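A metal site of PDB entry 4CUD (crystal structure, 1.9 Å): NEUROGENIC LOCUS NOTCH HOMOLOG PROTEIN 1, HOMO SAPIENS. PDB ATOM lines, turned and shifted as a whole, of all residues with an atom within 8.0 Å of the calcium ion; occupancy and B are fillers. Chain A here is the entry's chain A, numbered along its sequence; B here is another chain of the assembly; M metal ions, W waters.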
ATOM      1  N   PRO A  72      14.805  10.943  28.594  1.00  0.00           N
ATOM      2  CA  PRO A  72      13.727  11.915  28.365  1.00  0.00           C
ATOM      3  C   PRO A  72      12.344  11.290  28.576  1.00  0.00           C
ATOM      4  O   PRO A  72      12.111  10.141  28.209  1.00  0.00           O
ATOM      5  CB  PRO A  72      13.922  12.323  26.895  1.00  0.00           C
ATOM      6  CG  PRO A  72      15.379  12.054  26.625  1.00  0.00           C
ATOM      7  CD  PRO A  72      15.696  10.828  27.430  1.00  0.00           C
ATOM      8  N   GLY A  73      11.459  12.049  29.222  1.00  0.00           N
ATOM      9  CA  GLY A  73      10.122  11.554  29.537  1.00  0.00           C
ATOM     10  C   GLY A  73       9.988  11.010  30.939  1.00  0.00           C
ATOM     11  O   GLY A  73       8.878  10.778  31.405  1.00  0.00           O
ATOM     12  N   TYR A  74      11.117  10.837  31.632  1.00  0.00           N
ATOM     13  CA  TYR A  74      11.129  10.315  32.998  1.00  0.00           C
ATOM     14  C   TYR A  74      11.677  11.304  34.011  1.00  0.00           C
ATOM     15  O   TYR A  74      12.542  12.120  33.683  1.00  0.00           O
ATOM     16  CB  TYR A  74      11.901   8.997  33.068  1.00  0.00           C
ATOM     17  CG  TYR A  74      11.286   7.933  32.203  1.00  0.00           C
ATOM     18  CD1 TYR A  74      10.246   7.132  32.670  1.00  0.00           C
ATOM     19  CD2 TYR A  74      11.724   7.749  30.886  1.00  0.00           C
ATOM     20  CE1 TYR A  74       9.663   6.168  31.862  1.00  0.00           C
ATOM     21  CE2 TYR A  74      11.162   6.778  30.071  1.00  0.00           C
ATOM     22  CZ  TYR A  74      10.134   5.997  30.558  1.00  0.00           C
ATOM     23  OH  TYR A  74       9.569   5.048  29.748  1.00  0.00           O
ATOM     24  N   GLU A  75      11.163  11.220  35.227  1.00  0.00           N
ATOM     25  CA  GLU A  75      11.577  12.096  36.332  1.00  0.00           C
ATOM     26  C   GLU A  75      11.519  11.362  37.672  1.00  0.00           C
ATOM     27  O   GLU A  75      11.070  10.210  37.744  1.00  0.00           O
ATOM     28  CB  GLU A  75      10.702  13.366  36.365  1.00  0.00           C
ATOM     29  CG  GLU A  75       9.256  13.106  36.796  1.00  0.00           C
ATOM     30  CD  GLU A  75       8.376  14.352  36.774  1.00  0.00           C
ATOM     31  OE1 GLU A  75       7.814  14.701  35.716  1.00  0.00           O
ATOM     32  OE2 GLU A  75       8.247  14.994  37.823  1.00  0.00           O
ATOM     33  N   VAL A  81       9.080   7.981  37.528  1.00  0.00           N
ATOM     34  CA  VAL A  81       7.856   8.656  37.108  1.00  0.00           C
ATOM     35  C   VAL A  81       7.902   8.937  35.619  1.00  0.00           C
ATOM     36  O   VAL A  81       8.848   9.542  35.124  1.00  0.00           O
ATOM     37  CB  VAL A  81       7.629   9.957  37.894  1.00  0.00           C
ATOM     38  CG1 VAL A  81       6.494  10.760  37.288  1.00  0.00           C
ATOM     39  CG2 VAL A  81       7.353   9.632  39.357  1.00  0.00           C
ATOM     40  N   ASN A  82       6.885   8.447  34.914  1.00  0.00           N
ATOM     41  CA  ASN A  82       6.642   8.811  33.530  1.00  0.00           C
ATOM     42  C   ASN A  82       5.953  10.176  33.557  1.00  0.00           C
ATOM     43  O   ASN A  82       4.787  10.285  33.939  1.00  0.00           O
ATOM     44  CB  ASN A  82       5.753   7.750  32.855  1.00  0.00           C
ATOM     45  CG  ASN A  82       5.529   8.008  31.366  1.00  0.00           C
ATOM     46  OD1 ASN A  82       5.354   9.141  30.924  1.00  0.00           O
ATOM     47  ND2 ASN A  82       5.530   6.933  30.583  1.00  0.00           N
ATOM     48  N   THR A  83       6.689  11.222  33.211  1.00  0.00           N
ATOM     49  CA  THR A  83       6.151  12.578  33.232  1.00  0.00           C
ATOM     50  C   THR A  83       4.825  12.632  32.469  1.00  0.00           C
ATOM     51  O   THR A  83       4.718  12.090  31.368  1.00  0.00           O
ATOM     52  CB  THR A  83       7.134  13.590  32.620  1.00  0.00           C
ATOM     53  OG1 THR A  83       8.352  13.596  33.385  1.00  0.00           O
ATOM     54  CG2 THR A  83       6.529  14.993  32.616  1.00  0.00           C
ATOM     55  N   ASP A  84       3.801  13.248  33.069  1.00  0.00           N
ATOM     56  CA  ASP A  84       2.524  13.389  32.399  1.00  0.00           C
ATOM     57  C   ASP A  84       2.542  14.658  31.550  1.00  0.00           C
ATOM     58  O   ASP A  84       2.331  15.747  32.061  1.00  0.00           O
ATOM     59  CB  ASP A  84       1.384  13.405  33.434  1.00  0.00           C
ATOM     60  CG  ASP A  84      -0.008  13.475  32.805  1.00  0.00           C
ATOM     61  OD1 ASP A  84      -0.147  13.326  31.567  1.00  0.00           O
ATOM     62  OD2 ASP A  84      -0.967  13.682  33.564  1.00  0.00           O
ATOM     63  N   GLU A  85       2.827  14.506  30.258  1.00  0.00           N
ATOM     64  CA  GLU A  85       2.814  15.654  29.348  1.00  0.00           C
ATOM     65  C   GLU A  85       1.429  16.266  29.180  1.00  0.00           C
ATOM     66  O   GLU A  85       1.290  17.360  28.628  1.00  0.00           O
ATOM     67  CB  GLU A  85       3.441  15.295  28.003  1.00  0.00           C
ATOM     68  CG  GLU A  85       4.968  15.236  28.022  1.00  0.00           C
ATOM     69  CD  GLU A  85       5.523  13.914  28.531  1.00  0.00           C
ATOM     70  OE1 GLU A  85       4.833  12.886  28.436  1.00  0.00           O
ATOM     71  OE2 GLU A  85       6.669  13.898  29.027  1.00  0.00           O
ATOM     72  N   CYS A  86       0.403  15.578  29.667  1.00  0.00           N
ATOM     73  CA  CYS A  86      -0.958  16.096  29.571  1.00  0.00           C
ATOM     74  C   CYS A  86      -1.308  17.021  30.725  1.00  0.00           C
ATOM     75  O   CYS A  86      -2.327  17.732  30.672  1.00  0.00           O
ATOM     76  CB  CYS A  86      -1.978  14.955  29.447  1.00  0.00           C
ATOM     77  SG  CYS A  86      -1.784  14.091  27.869  1.00  0.00           S
ATOM     78  N   LEU A  98      -3.612  12.300  25.224  1.00  0.00           N
ATOM     79  CA  LEU A  98      -3.066  10.972  25.477  1.00  0.00           C
ATOM     80  C   LEU A  98      -1.594  11.097  25.816  1.00  0.00           C
ATOM     81  O   LEU A  98      -0.820  11.632  25.027  1.00  0.00           O
ATOM     82  CB  LEU A  98      -3.222  10.091  24.239  1.00  0.00           C
ATOM     83  CG  LEU A  98      -4.568  10.019  23.528  1.00  0.00           C
ATOM     84  CD1 LEU A  98      -4.445   9.166  22.268  1.00  0.00           C
ATOM     85  CD2 LEU A  98      -5.635   9.467  24.452  1.00  0.00           C
ATOM     86  N   ASP A  99      -1.214  10.598  26.991  1.00  0.00           N
ATOM     87  CA  ASP A  99       0.176  10.700  27.430  1.00  0.00           C
ATOM     88  C   ASP A  99       1.044   9.624  26.786  1.00  0.00           C
ATOM     89  O   ASP A  99       0.649   8.468  26.710  1.00  0.00           O
ATOM     90  CB  ASP A  99       0.301  10.594  28.942  1.00  0.00           C
ATOM     91  CG  ASP A  99       1.735  10.811  29.415  1.00  0.00           C
ATOM     92  OD1 ASP A  99       2.258  11.923  29.212  1.00  0.00           O
ATOM     93  OD2 ASP A  99       2.338   9.874  29.958  1.00  0.00           O
ATOM     94  N   LYS A 100       2.226  10.014  26.323  1.00  0.00           N
ATOM     95  CA  LYS A 100       3.200   9.072  25.769  1.00  0.00           C
ATOM     96  C   LYS A 100       4.555   9.316  26.445  1.00  0.00           C
ATOM     97  O   LYS A 100       4.621   9.947  27.489  1.00  0.00           O
ATOM     98  CB  LYS A 100       3.302   9.233  24.261  1.00  0.00           C
ATOM     99  CG  LYS A 100       1.998   9.011  23.498  1.00  0.00           C
ATOM    100  CD  LYS A 100       2.320   8.652  22.066  1.00  0.00           C
ATOM    101  CE  LYS A 100       1.077   8.268  21.288  1.00  0.00           C
ATOM    102  NZ  LYS A 100       1.461   7.735  19.948  1.00  0.00           N
ATOM    103  N   ILE A 101       5.630   8.811  25.844  1.00  0.00           N
ATOM    104  CA  ILE A 101       6.955   9.014  26.431  1.00  0.00           C
ATOM    105  C   ILE A 101       7.581  10.289  25.869  1.00  0.00           C
ATOM    106  O   ILE A 101       7.853  10.376  24.672  1.00  0.00           O
ATOM    107  CB  ILE A 101       7.887   7.779  26.240  1.00  0.00           C
ATOM    108  CG1 ILE A 101       7.265   6.529  26.886  1.00  0.00           C
ATOM    109  CG2 ILE A 101       9.243   8.050  26.879  1.00  0.00           C
ATOM    110  CD1 ILE A 101       7.972   5.229  26.549  1.00  0.00           C
ATOM    111  N   ASN A 102       7.776  11.287  26.729  1.00  0.00           N
ATOM    112  CA  ASN A 102       8.295  12.614  26.333  1.00  0.00           C
ATOM    113  C   ASN A 102       7.545  13.241  25.153  1.00  0.00           C
ATOM    114  O   ASN A 102       8.103  14.008  24.346  1.00  0.00           O
ATOM    115  CB  ASN A 102       9.814  12.556  26.068  1.00  0.00           C
ATOM    116  CG  ASN A 102      10.466  13.933  26.122  1.00  0.00           C
ATOM    117  OD1 ASN A 102      10.091  14.789  26.941  1.00  0.00           O
ATOM    118  ND2 ASN A 102      11.430  14.153  25.252  1.00  0.00           N
ATOM    119  N   GLU A 103       6.255  12.912  25.079  1.00  0.00           N
ATOM    120  CA  GLU A 103       5.379  13.289  23.989  1.00  0.00           C
ATOM    121  C   GLU A 103       3.925  13.083  24.423  1.00  0.00           C
ATOM    122  O   GLU A 103       3.656  12.431  25.422  1.00  0.00           O
ATOM    123  CB  GLU A 103       5.693  12.439  22.744  1.00  0.00           C
ATOM    124  CG  GLU A 103       4.955  12.850  21.489  1.00  0.00           C
ATOM    125  CD  GLU A 103       5.166  14.324  21.143  1.00  0.00           C
ATOM    126  OE1 GLU A 103       6.202  14.647  20.528  1.00  0.00           O
ATOM    127  OE2 GLU A 103       4.301  15.160  21.507  1.00  0.00           O
ATOM    128  N   PHE A 104       3.002  13.674  23.664  1.00  0.00           N
ATOM    129  CA  PHE A 104       1.571  13.508  23.889  1.00  0.00           C
ATOM    130  C   PHE A 104       0.853  13.566  22.555  1.00  0.00           C
ATOM    131  O   PHE A 104       1.395  14.064  21.562  1.00  0.00           O
ATOM    132  CB  PHE A 104       1.034  14.593  24.846  1.00  0.00           C
ATOM    133  CG  PHE A 104       1.128  15.986  24.264  1.00  0.00           C
ATOM    134  CD1 PHE A 104       0.080  16.517  23.516  1.00  0.00           C
ATOM    135  CD2 PHE A 104       2.264  16.771  24.479  1.00  0.00           C
ATOM    136  CE1 PHE A 104       0.164  17.791  22.965  1.00  0.00           C
ATOM    137  CE2 PHE A 104       2.362  18.041  23.929  1.00  0.00           C
ATOM    138  CZ  PHE A 104       1.315  18.551  23.175  1.00  0.00           C
ATOM    139  N   GLN B 118       8.371  20.833  31.795  1.00  0.00           N
ATOM    140  CA  GLN B 118       7.597  20.537  32.999  1.00  0.00           C
ATOM    141  C   GLN B 118       8.420  20.193  34.213  1.00  0.00           C
ATOM    142  O   GLN B 118       8.017  20.468  35.346  1.00  0.00           O
ATOM    143  CB  GLN B 118       6.744  19.293  32.770  1.00  0.00           C
ATOM    144  CG  GLN B 118       5.386  19.522  32.164  1.00  0.00           C
ATOM    145  CD  GLN B 118       4.730  18.193  31.901  1.00  0.00           C
ATOM    146  OE1 GLN B 118       4.663  17.741  30.765  1.00  0.00           O
ATOM    147  NE2 GLN B 118       4.275  17.532  32.963  1.00  0.00           N
HETATM  148 CA    CA M   1       4.585  10.849  29.562  1.00  0.00          CA
HETATM  149  O   HOH W   1       6.948  11.231  29.424  1.00  0.00           O
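Water W1 lies within hydrogen-bond range of OE2 of Glu 85 (2.7 Å), O of Gly 73 (2.8 Å) and N of Asn 102 (2.8 Å).
The calcium ion is bound by O of Thr 83 (2.2 Å), O of Lys 100 (2.3 Å), OD1 of Asn 82 (2.3 Å), OE1 of Glu 85 (2.3 Å), water W1 (2.4 Å), OD2 of Asp 99 (2.5 Å) and OD1 of Asp 99 (2.6 Å).
The calcium ion has seven donor atoms within binding distance.
The backbone NH of Thr 83 sits at hydrogen-bond distance from the backbone carbonyl oxygen of Gly 73.
OG1 of Thr 83 lies within hydrogen-bond range of OE1 of Glu 75 (2.6 Å).
SG of Cys 86 is in hydrogen-bond range of N of Asp 99 (3.6 Å).
Five residues have an atom within 4 Å of the calcium ion: Asn 82, Thr 83, Glu 85, Asp 99 and Lys 100.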
